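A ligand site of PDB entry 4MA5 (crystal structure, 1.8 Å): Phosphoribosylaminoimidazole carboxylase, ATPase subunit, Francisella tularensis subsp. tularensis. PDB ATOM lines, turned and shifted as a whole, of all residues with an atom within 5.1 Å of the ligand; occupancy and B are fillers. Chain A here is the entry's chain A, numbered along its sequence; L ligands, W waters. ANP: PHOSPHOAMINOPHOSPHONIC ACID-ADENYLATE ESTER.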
ATOM      1  N   ARG A  98     -11.421  16.312  25.269  1.00  0.00           N
ATOM      2  CA  ARG A  98     -10.038  16.735  25.121  1.00  0.00           C
ATOM      3  C   ARG A  98      -9.032  15.589  24.987  1.00  0.00           C
ATOM      4  O   ARG A  98      -8.036  15.722  24.255  1.00  0.00           O
ATOM      5  CB  ARG A  98      -9.634  17.671  26.255  1.00  0.00           C
ATOM      6  CG  ARG A  98     -10.433  18.983  26.260  1.00  0.00           C
ATOM      7  CD  ARG A  98     -10.018  19.928  27.374  1.00  0.00           C
ATOM      8  NE  ARG A  98     -10.771  21.179  27.258  1.00  0.00           N
ATOM      9  CZ  ARG A  98     -11.988  21.372  27.767  1.00  0.00           C
ATOM     10  NH1 ARG A  98     -12.604  22.529  27.618  1.00  0.00           N
ATOM     11  NH2 ARG A  98     -12.603  20.391  28.435  1.00  0.00           N
ATOM     12  N   ALA A 113      -0.011  19.979  22.515  1.00  0.00           N
ATOM     13  CA  ALA A 113       0.566  20.084  23.844  1.00  0.00           C
ATOM     14  C   ALA A 113       0.752  18.668  24.373  1.00  0.00           C
ATOM     15  O   ALA A 113      -0.026  17.775  24.041  1.00  0.00           O
ATOM     16  CB  ALA A 113      -0.361  20.862  24.769  1.00  0.00           C
ATOM     17  N   ILE A 136      -1.837  22.672  32.983  1.00  0.00           N
ATOM     18  CA  ILE A 136      -3.237  22.882  33.308  1.00  0.00           C
ATOM     19  C   ILE A 136      -3.897  21.533  33.544  1.00  0.00           C
ATOM     20  O   ILE A 136      -3.710  20.604  32.759  1.00  0.00           O
ATOM     21  CB  ILE A 136      -3.987  23.607  32.180  1.00  0.00           C
ATOM     22  CG1 ILE A 136      -3.224  24.843  31.681  1.00  0.00           C
ATOM     23  CG2 ILE A 136      -5.390  24.001  32.635  1.00  0.00           C
ATOM     24  CD1 ILE A 136      -3.808  25.445  30.402  1.00  0.00           C
ATOM     25  N   LYS A 138      -7.385  20.058  33.203  1.00  0.00           N
ATOM     26  CA  LYS A 138      -8.674  20.378  32.584  1.00  0.00           C
ATOM     27  C   LYS A 138      -9.622  19.207  32.678  1.00  0.00           C
ATOM     28  O   LYS A 138      -9.203  18.050  32.787  1.00  0.00           O
ATOM     29  CB  LYS A 138      -8.495  20.676  31.099  1.00  0.00           C
ATOM     30  CG  LYS A 138      -7.475  21.734  30.759  1.00  0.00           C
ATOM     31  CD  LYS A 138      -7.534  21.958  29.246  1.00  0.00           C
ATOM     32  CE  LYS A 138      -6.585  23.050  28.794  1.00  0.00           C
ATOM     33  NZ  LYS A 138      -6.704  23.185  27.312  1.00  0.00           N
ATOM     34  N   GLY A 143     -16.555  22.889  30.134  1.00  0.00           N
ATOM     35  CA  GLY A 143     -15.757  24.097  30.073  1.00  0.00           C
ATOM     36  C   GLY A 143     -15.816  24.897  28.801  1.00  0.00           C
ATOM     37  O   GLY A 143     -15.757  24.384  27.673  1.00  0.00           O
ATOM     38  N   TYR A 144     -15.922  26.204  29.016  1.00  0.00           N
ATOM     39  CA  TYR A 144     -15.942  27.186  27.958  1.00  0.00           C
ATOM     40  C   TYR A 144     -15.027  28.313  28.411  1.00  0.00           C
ATOM     41  O   TYR A 144     -14.991  28.637  29.609  1.00  0.00           O
ATOM     42  CB  TYR A 144     -17.351  27.749  27.777  1.00  0.00           C
ATOM     43  CG  TYR A 144     -18.385  26.725  27.366  1.00  0.00           C
ATOM     44  CD1 TYR A 144     -18.711  26.522  26.033  1.00  0.00           C
ATOM     45  CD2 TYR A 144     -19.066  25.969  28.317  1.00  0.00           C
ATOM     46  CE1 TYR A 144     -19.674  25.594  25.643  1.00  0.00           C
ATOM     47  CE2 TYR A 144     -20.023  25.031  27.946  1.00  0.00           C
ATOM     48  CZ  TYR A 144     -20.318  24.844  26.602  1.00  0.00           C
ATOM     49  OH  TYR A 144     -21.274  23.922  26.213  1.00  0.00           O
ATOM     50  N   ASP A 145     -14.305  28.878  27.451  1.00  0.00           N
ATOM     51  CA  ASP A 145     -13.539  30.121  27.635  1.00  0.00           C
ATOM     52  C   ASP A 145     -12.693  30.179  28.907  1.00  0.00           C
ATOM     53  O   ASP A 145     -12.718  31.171  29.656  1.00  0.00           O
ATOM     54  CB  ASP A 145     -14.461  31.340  27.505  1.00  0.00           C
ATOM     55  CG  ASP A 145     -15.222  31.350  26.188  1.00  0.00           C
ATOM     56  OD1 ASP A 145     -14.613  31.039  25.141  1.00  0.00           O
ATOM     57  OD2 ASP A 145     -16.426  31.663  26.207  1.00  0.00           O
ATOM     58  N   GLY A 146     -11.963  29.089  29.148  1.00  0.00           N
ATOM     59  CA  GLY A 146     -10.994  29.045  30.224  1.00  0.00           C
ATOM     60  C   GLY A 146     -11.575  28.615  31.557  1.00  0.00           C
ATOM     61  O   GLY A 146     -10.857  28.572  32.561  1.00  0.00           O
ATOM     62  N   LYS A 147     -12.863  28.296  31.582  1.00  0.00           N
ATOM     63  CA  LYS A 147     -13.492  27.951  32.859  1.00  0.00           C
ATOM     64  C   LYS A 147     -13.477  26.441  33.080  1.00  0.00           C
ATOM     65  O   LYS A 147     -13.321  25.675  32.128  1.00  0.00           O
ATOM     66  CB  LYS A 147     -14.922  28.492  32.937  1.00  0.00           C
ATOM     67  CG  LYS A 147     -15.048  30.008  32.915  1.00  0.00           C
ATOM     68  N   GLN A 149     -11.249  24.661  34.892  1.00  0.00           N
ATOM     69  CA  GLN A 149      -9.896  24.111  34.868  1.00  0.00           C
ATOM     70  C   GLN A 149      -9.083  24.706  35.991  1.00  0.00           C
ATOM     71  O   GLN A 149      -9.579  25.558  36.743  1.00  0.00           O
ATOM     72  CB  GLN A 149      -9.226  24.401  33.537  1.00  0.00           C
ATOM     73  CG  GLN A 149      -9.061  25.887  33.211  1.00  0.00           C
ATOM     74  CD  GLN A 149      -8.481  26.094  31.820  1.00  0.00           C
ATOM     75  OE1 GLN A 149      -8.547  25.211  30.959  1.00  0.00           O
ATOM     76  NE2 GLN A 149      -7.918  27.268  31.587  1.00  0.00           N
ATOM     77  N   GLU A 175      -2.553  18.991  30.683  1.00  0.00           N
ATOM     78  CA  GLU A 175      -1.899  19.543  29.496  1.00  0.00           C
ATOM     79  C   GLU A 175      -0.732  20.400  29.906  1.00  0.00           C
ATOM     80  O   GLU A 175      -0.867  21.244  30.798  1.00  0.00           O
ATOM     81  CB  GLU A 175      -2.849  20.419  28.683  1.00  0.00           C
ATOM     82  CG  GLU A 175      -3.988  19.688  28.018  1.00  0.00           C
ATOM     83  CD  GLU A 175      -4.745  20.579  27.059  1.00  0.00           C
ATOM     84  OE1 GLU A 175      -4.209  21.653  26.699  1.00  0.00           O
ATOM     85  OE2 GLU A 175      -5.861  20.200  26.662  1.00  0.00           O
ATOM     86  N   ALA A 176       0.414  20.205  29.262  1.00  0.00           N
ATOM     87  CA  ALA A 176       1.540  21.117  29.463  1.00  0.00           C
ATOM     88  C   ALA A 176       1.149  22.491  28.927  1.00  0.00           C
ATOM     89  O   ALA A 176       0.455  22.596  27.917  1.00  0.00           O
ATOM     90  CB  ALA A 176       2.778  20.596  28.764  1.00  0.00           C
ATOM     91  N   PHE A 177       1.548  23.535  29.650  1.00  0.00           N
ATOM     92  CA  PHE A 177       1.215  24.893  29.261  1.00  0.00           C
ATOM     93  C   PHE A 177       2.142  25.302  28.123  1.00  0.00           C
ATOM     94  O   PHE A 177       3.352  25.425  28.321  1.00  0.00           O
ATOM     95  CB  PHE A 177       1.392  25.837  30.454  1.00  0.00           C
ATOM     96  CG  PHE A 177       0.553  27.078  30.377  1.00  0.00           C
ATOM     97  CD1 PHE A 177       0.903  28.123  29.535  1.00  0.00           C
ATOM     98  CD2 PHE A 177      -0.583  27.207  31.156  1.00  0.00           C
ATOM     99  CE1 PHE A 177       0.126  29.274  29.475  1.00  0.00           C
ATOM    100  CE2 PHE A 177      -1.361  28.358  31.096  1.00  0.00           C
ATOM    101  CZ  PHE A 177      -1.007  29.387  30.250  1.00  0.00           C
ATOM    102  N   VAL A 178       1.584  25.495  26.945  1.00  0.00           N
ATOM    103  CA  VAL A 178       2.368  25.853  25.765  1.00  0.00           C
ATOM    104  C   VAL A 178       2.735  27.335  25.808  1.00  0.00           C
ATOM    105  O   VAL A 178       1.866  28.195  26.020  1.00  0.00           O
ATOM    106  CB  VAL A 178       1.601  25.548  24.452  1.00  0.00           C
ATOM    107  CG1 VAL A 178       2.358  26.053  23.232  1.00  0.00           C
ATOM    108  CG2 VAL A 178       1.313  24.050  24.327  1.00  0.00           C
ATOM    109  N   PHE A 180       3.403  29.956  23.668  1.00  0.00           N
ATOM    110  CA  PHE A 180       3.329  30.287  22.243  1.00  0.00           C
ATOM    111  C   PHE A 180       3.723  31.720  21.935  1.00  0.00           C
ATOM    112  O   PHE A 180       3.667  32.604  22.810  1.00  0.00           O
ATOM    113  CB  PHE A 180       1.928  29.991  21.679  1.00  0.00           C
ATOM    114  CG  PHE A 180       0.800  30.599  22.461  1.00  0.00           C
ATOM    115  CD1 PHE A 180       0.384  31.894  22.213  1.00  0.00           C
ATOM    116  CD2 PHE A 180       0.158  29.895  23.454  1.00  0.00           C
ATOM    117  CE1 PHE A 180      -0.648  32.464  22.943  1.00  0.00           C
ATOM    118  CE2 PHE A 180      -0.876  30.455  24.174  1.00  0.00           C
ATOM    119  CZ  PHE A 180      -1.271  31.732  23.920  1.00  0.00           C
ATOM    120  N   GLU A 183      -1.274  32.955  18.171  1.00  0.00           N
ATOM    121  CA  GLU A 183      -2.259  31.933  17.859  1.00  0.00           C
ATOM    122  C   GLU A 183      -2.878  32.196  16.491  1.00  0.00           C
ATOM    123  O   GLU A 183      -3.064  33.358  16.107  1.00  0.00           O
ATOM    124  CB  GLU A 183      -3.388  31.932  18.890  1.00  0.00           C
ATOM    125  CG  GLU A 183      -2.969  31.612  20.305  1.00  0.00           C
ATOM    126  CD  GLU A 183      -4.162  31.596  21.233  1.00  0.00           C
ATOM    127  OE1 GLU A 183      -4.504  32.662  21.799  1.00  0.00           O
ATOM    128  OE2 GLU A 183      -4.773  30.524  21.393  1.00  0.00           O
ATOM    129  N   HIS A 206      -6.411  36.134  22.529  1.00  0.00           N
ATOM    130  CA  HIS A 206      -7.277  35.771  23.639  1.00  0.00           C
ATOM    131  C   HIS A 206      -6.969  36.648  24.822  1.00  0.00           C
ATOM    132  O   HIS A 206      -5.816  37.031  25.034  1.00  0.00           O
ATOM    133  CB  HIS A 206      -7.084  34.308  24.031  1.00  0.00           C
ATOM    134  CG  HIS A 206      -7.787  33.339  23.132  1.00  0.00           C
ATOM    135  ND1 HIS A 206      -7.162  32.722  22.075  1.00  0.00           N
ATOM    136  CD2 HIS A 206      -9.069  32.894  23.130  1.00  0.00           C
ATOM    137  CE1 HIS A 206      -8.024  31.927  21.458  1.00  0.00           C
ATOM    138  NE2 HIS A 206      -9.185  32.015  22.082  1.00  0.00           N
ATOM    139  N   GLY A 209      -8.967  33.942  28.495  1.00  0.00           N
ATOM    140  CA  GLY A 209      -9.607  32.723  28.038  1.00  0.00           C
ATOM    141  C   GLY A 209     -10.618  32.939  26.929  1.00  0.00           C
ATOM    142  O   GLY A 209     -11.177  31.982  26.384  1.00  0.00           O
ATOM    143  N   ILE A 211     -11.723  34.912  23.215  1.00  0.00           N
ATOM    144  CA  ILE A 211     -11.219  35.576  22.036  1.00  0.00           C
ATOM    145  C   ILE A 211     -11.721  37.019  22.001  1.00  0.00           C
ATOM    146  O   ILE A 211     -12.908  37.285  22.227  1.00  0.00           O
ATOM    147  CB  ILE A 211     -11.614  34.750  20.799  1.00  0.00           C
ATOM    148  CG1 ILE A 211     -10.805  35.151  19.570  1.00  0.00           C
ATOM    149  CG2 ILE A 211     -13.106  34.755  20.599  1.00  0.00           C
ATOM    150  CD1 ILE A 211     -10.642  34.008  18.591  1.00  0.00           C
ATOM    151  N   GLU A 247      -7.906  25.499  15.795  1.00  0.00           N
ATOM    152  CA  GLU A 247      -7.098  26.502  16.456  1.00  0.00           C
ATOM    153  C   GLU A 247      -5.696  25.973  16.705  1.00  0.00           C
ATOM    154  O   GLU A 247      -5.535  24.825  17.131  1.00  0.00           O
ATOM    155  CB  GLU A 247      -7.746  26.934  17.765  1.00  0.00           C
ATOM    156  CG  GLU A 247      -9.046  27.686  17.583  1.00  0.00           C
ATOM    157  CD  GLU A 247      -9.545  28.243  18.888  1.00  0.00           C
ATOM    158  OE1 GLU A 247     -10.009  27.434  19.718  1.00  0.00           O
ATOM    159  OE2 GLU A 247      -9.452  29.463  19.089  1.00  0.00           O
ATOM    160  N   PHE A 249      -1.454  26.840  18.066  1.00  0.00           N
ATOM    161  CA  PHE A 249      -0.427  27.665  18.659  1.00  0.00           C
ATOM    162  C   PHE A 249       0.684  27.771  17.606  1.00  0.00           C
ATOM    163  O   PHE A 249       0.901  26.837  16.841  1.00  0.00           O
ATOM    164  CB  PHE A 249       0.156  27.013  19.919  1.00  0.00           C
ATOM    165  CG  PHE A 249      -0.860  26.703  20.985  1.00  0.00           C
ATOM    166  CD1 PHE A 249      -1.604  27.718  21.553  1.00  0.00           C
ATOM    167  CD2 PHE A 249      -1.046  25.407  21.428  1.00  0.00           C
ATOM    168  CE1 PHE A 249      -2.542  27.432  22.549  1.00  0.00           C
ATOM    169  CE2 PHE A 249      -1.973  25.125  22.417  1.00  0.00           C
ATOM    170  CZ  PHE A 249      -2.712  26.137  22.977  1.00  0.00           C
ATOM    171  N   ASN A 258      -4.149  23.228  19.010  1.00  0.00           N
ATOM    172  CA  ASN A 258      -4.734  23.547  20.307  1.00  0.00           C
ATOM    173  C   ASN A 258      -6.034  22.762  20.480  1.00  0.00           C
ATOM    174  O   ASN A 258      -6.128  21.864  21.324  1.00  0.00           O
ATOM    175  CB  ASN A 258      -5.003  25.047  20.340  1.00  0.00           C
ATOM    176  CG  ASN A 258      -5.741  25.494  21.592  1.00  0.00           C
ATOM    177  OD1 ASN A 258      -5.903  24.735  22.542  1.00  0.00           O
ATOM    178  ND2 ASN A 258      -6.186  26.750  21.592  1.00  0.00           N
ATOM    179  N   GLU A 259      -7.026  23.080  19.660  1.00  0.00           N
ATOM    180  CA  GLU A 259      -8.277  22.323  19.684  1.00  0.00           C
ATOM    181  C   GLU A 259      -9.044  22.516  18.386  1.00  0.00           C
ATOM    182  O   GLU A 259      -8.703  23.369  17.568  1.00  0.00           O
ATOM    183  CB  GLU A 259      -9.144  22.767  20.862  1.00  0.00           C
ATOM    184  CG  GLU A 259      -9.628  24.184  20.738  1.00  0.00           C
ATOM    185  CD  GLU A 259     -10.678  24.507  21.792  1.00  0.00           C
ATOM    186  OE1 GLU A 259     -11.746  23.845  21.793  1.00  0.00           O
ATOM    187  OE2 GLU A 259     -10.446  25.411  22.598  1.00  0.00           O
ATOM    188  N   ARG A 263     -17.733  23.225  13.658  1.00  0.00           N
ATOM    189  CA  ARG A 263     -18.784  24.218  13.468  1.00  0.00           C
ATOM    190  C   ARG A 263     -18.183  25.527  13.019  1.00  0.00           C
ATOM    191  O   ARG A 263     -16.965  25.692  13.053  1.00  0.00           O
ATOM    192  CB  ARG A 263     -19.542  24.447  14.780  1.00  0.00           C
ATOM    193  CG  ARG A 263     -18.605  24.741  15.978  1.00  0.00           C
ATOM    194  CD  ARG A 263     -19.381  25.284  17.140  1.00  0.00           C
ATOM    195  NE  ARG A 263     -18.573  25.460  18.351  1.00  0.00           N
ATOM    196  CZ  ARG A 263     -17.839  26.538  18.596  1.00  0.00           C
ATOM    197  NH1 ARG A 263     -17.791  27.531  17.706  1.00  0.00           N
ATOM    198  NH2 ARG A 263     -17.140  26.642  19.719  1.00  0.00           N
ATOM    199  N   HIS A 265     -17.139  29.244  13.816  1.00  0.00           N
ATOM    200  CA  HIS A 265     -16.364  29.570  14.994  1.00  0.00           C
ATOM    201  C   HIS A 265     -16.138  31.067  15.072  1.00  0.00           C
ATOM    202  O   HIS A 265     -16.081  31.733  14.044  1.00  0.00           O
ATOM    203  CB  HIS A 265     -14.999  28.890  14.876  1.00  0.00           C
ATOM    204  CG  HIS A 265     -14.204  28.914  16.142  1.00  0.00           C
ATOM    205  ND1 HIS A 265     -13.163  29.793  16.353  1.00  0.00           N
ATOM    206  CD2 HIS A 265     -14.272  28.142  17.259  1.00  0.00           C
ATOM    207  CE1 HIS A 265     -12.642  29.577  17.541  1.00  0.00           C
ATOM    208  NE2 HIS A 265     -13.283  28.586  18.113  1.00  0.00           N
ATOM    209  N   LYS A 335     -20.635  36.584  25.312  1.00  0.00           N
ATOM    210  CA  LYS A 335     -20.487  37.121  23.959  1.00  0.00           C
ATOM    211  C   LYS A 335     -21.800  37.722  23.497  1.00  0.00           C
ATOM    212  O   LYS A 335     -22.790  36.993  23.337  1.00  0.00           O
ATOM    213  CB  LYS A 335     -20.033  36.020  22.989  1.00  0.00           C
ATOM    214  CG  LYS A 335     -18.609  35.545  23.281  1.00  0.00           C
ATOM    215  CD  LYS A 335     -18.238  34.286  22.508  1.00  0.00           C
ATOM    216  CE  LYS A 335     -16.803  33.892  22.827  1.00  0.00           C
ATOM    217  NZ  LYS A 335     -16.243  32.845  21.924  1.00  0.00           N
HETATM  218  PG  ANP L   1     -12.011  29.204  22.132  1.00  0.00           P
HETATM  219  O1G ANP L   1     -10.686  28.508  22.129  1.00  0.00           O
HETATM  220  O2G ANP L   1     -12.920  28.606  20.992  1.00  0.00           O
HETATM  221  O3G ANP L   1     -11.808  30.747  21.894  1.00  0.00           O
HETATM  222  PB  ANP L   1     -12.881  27.541  24.392  1.00  0.00           P
HETATM  223  O1B ANP L   1     -14.286  27.313  24.836  1.00  0.00           O
HETATM  224  O2B ANP L   1     -12.472  26.345  23.487  1.00  0.00           O
HETATM  225  N3B ANP L   1     -12.810  29.044  23.622  1.00  0.00           N
HETATM  226  PA  ANP L   1     -10.874  26.660  26.163  1.00  0.00           P
HETATM  227  O1A ANP L   1     -11.033  25.342  25.536  1.00  0.00           O
HETATM  228  O2A ANP L   1     -10.995  26.633  27.686  1.00  0.00           O
HETATM  229  O3A ANP L   1     -11.979  27.670  25.673  1.00  0.00           O
HETATM  230  O5' ANP L   1      -9.511  27.333  25.715  1.00  0.00           O
HETATM  231  C5' ANP L   1      -9.387  28.755  25.939  1.00  0.00           C
HETATM  232  C4' ANP L   1      -8.049  29.309  25.505  1.00  0.00           C
HETATM  233  O4' ANP L   1      -7.034  29.016  26.498  1.00  0.00           O
HETATM  234  C3' ANP L   1      -7.465  28.768  24.208  1.00  0.00           C
HETATM  235  O3' ANP L   1      -8.037  29.388  23.049  1.00  0.00           O
HETATM  236  C2' ANP L   1      -5.977  29.068  24.364  1.00  0.00           C
HETATM  237  O2' ANP L   1      -5.628  30.387  23.948  1.00  0.00           O
HETATM  238  C1' ANP L   1      -5.765  28.910  25.871  1.00  0.00           C
HETATM  239  N9  ANP L   1      -5.191  27.616  26.198  1.00  0.00           N
HETATM  240  C8  ANP L   1      -5.837  26.403  26.264  1.00  0.00           C
HETATM  241  N7  ANP L   1      -5.044  25.388  26.529  1.00  0.00           N
HETATM  242  C5  ANP L   1      -3.795  25.964  26.648  1.00  0.00           C
HETATM  243  C6  ANP L   1      -2.519  25.435  26.934  1.00  0.00           C
HETATM  244  N6  ANP L   1      -2.298  24.136  27.155  1.00  0.00           N
HETATM  245  N1  ANP L   1      -1.467  26.286  26.968  1.00  0.00           N
HETATM  246  C2  ANP L   1      -1.688  27.589  26.733  1.00  0.00           C
HETATM  247  N3  ANP L   1      -2.842  28.207  26.465  1.00  0.00           N
HETATM  248  C4  ANP L   1      -3.860  27.339  26.431  1.00  0.00           C
HETATM  249  O   HOH W   1     -13.872  24.143  23.172  1.00  0.00           O
HETATM  250  O   HOH W   2      -7.987  24.371  24.417  1.00  0.00           O
HETATM  251  O   HOH W   3     -12.591  25.353  29.605  1.00  0.00           O
HETATM  252  O   HOH W   4      -4.594  32.183  25.964  1.00  0.00           O
HETATM  253  O   HOH W   5     -15.451  28.965  21.061  1.00  0.00           O
HETATM  254  O   HOH W   6     -13.563  32.390  22.956  1.00  0.00           O
HETATM  255  O   HOH W   7     -15.182  24.886  25.041  1.00  0.00           O
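An oxygen (O2B) of the ligand lies close to the side-chain carboxylate of Glu 259, 2.4 Å away.
The side-chain carboxylate (OE2) of Glu 183 is in hydrogen-bond range of an oxygen (O2') of the ligand (2.7 Å).
OE1 of Glu 247 sits close to O1G of the ligand (2.7 Å).
The side-chain amino group (NZ) of Lys 138 is in hydrogen-bond range of a nitrogen (N7) of the ligand, 2.9 Å away.
O2G of the ligand lies within hydrogen-bond range of NE2 of His 265, at 2.9 Å.
NE2 of His 206 is in hydrogen-bond range of O3G of the ligand.
N of Gly 146 sits at hydrogen-bond distance from O2A of the ligand (3.0 Å).
N of Asp 145 is in hydrogen-bond range of O1B of the ligand (3.0 Å).
N3B of the ligand lies within hydrogen-bond range of OD1 of Asp 145.
N1 of the ligand lies within hydrogen-bond range of N of Val 178.
OE1 of Glu 175 lies within hydrogen-bond range of N6 of the ligand, at 3.2 Å.
The backbone carbonyl oxygen (O) of Ala 176 is in hydrogen-bond range of a nitrogen (N6) of the ligand, at 3.2 Å.
The guanidinium group of Arg 98 lies within salt-bridge range of an oxygen (O1A) of the ligand, at 3.8 Å.
The backbone NH (N) of Glu 247 sits at hydrogen-bond distance from the backbone carbonyl oxygen (O) of Glu 259 (2.9 Å).
A ring nitrogen (ND1) of His 206 is in hydrogen-bond range of the side-chain carboxylate of Glu 183 (2.7 Å).
The backbone carbonyl oxygen (O) of Glu 247 is in hydrogen-bond range of the backbone NH (N) of Asn 258.
The side-chain amino group (NZ) of Lys 138 lies within salt-bridge range of the side-chain carboxylate (OE1) of Glu 175, at 3.0 Å.
O of Gly 146 sits close to NE2 of Gln 149 (3.4 Å).
The backbone NH of Ile 136 is in hydrogen-bond range of the backbone carbonyl oxygen of Glu 175 (2.8 Å).
CD1 of Ile 136 touches C6 of the ligand, 3.7 Å away.
CA of Tyr 144 touches O1B of the ligand, 3.5 Å away.
Phe 177 touches the ligand (CE1 to C2, 3.7 Å).
Phe 180 touches the ligand.
Gly 209 touches the ligand.
Phe 249 touches the ligand.
Asn 258 touches the ligand (ND2 to O3', 3.5 Å).
Hydrophobic or aromatic side chains that line the ligand: Ile 136, Phe 177, Phe 180, His 206, Phe 249 and His 265.
Within 4 Å of the ligand: Arg 98, Ile 136, Lys 138, Tyr 144, Asp 145, Gly 146, Glu 175, Ala 176, Phe 177, Val 178, Phe 180, Glu 183, His 206, Gly 209, Glu 247, Phe 249, Asn 258, Glu 259 and His 265.
Water W5 lies within hydrogen-bond range of O2G of the ligand (2.6 Å) and NH2 of Arg 263 (3.2 Å).
Water W7 bridges an oxygen (O1B) of the ligand (2.6 Å) and the backbone carbonyl oxygen (O) of Gly 143 (2.7 Å).
Water W6 lies within hydrogen-bond range of an oxygen (O3G) of the ligand (2.6 Å), the side-chain carboxylate (OD1) of Asp 145 (2.8 Å), the side-chain amino group (NZ) of Lys 335 (2.9 Å) and the backbone NH (N) of Ile 211 (3.1 Å).
Water W1 lies within hydrogen-bond range of the side-chain carboxylate of Glu 259 (2.6 Å) and an oxygen (O2B) of the ligand (2.6 Å).
Water W3 lies within hydrogen-bond range of the backbone carbonyl oxygen of Lys 147 (2.6 Å), an oxygen (O2A) of the ligand (2.8 Å), the guanidinium group of Arg 98 (3.5 Å) and the backbone NH of Tyr 144 (3.5 Å).
Water W2 lies within hydrogen-bond range of OD1 of Asn 258 (2.8 Å), OE2 of Glu 259 (3.2 Å), NZ of Lys 138 (3.4 Å) and O1A of the ligand (3.4 Å).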
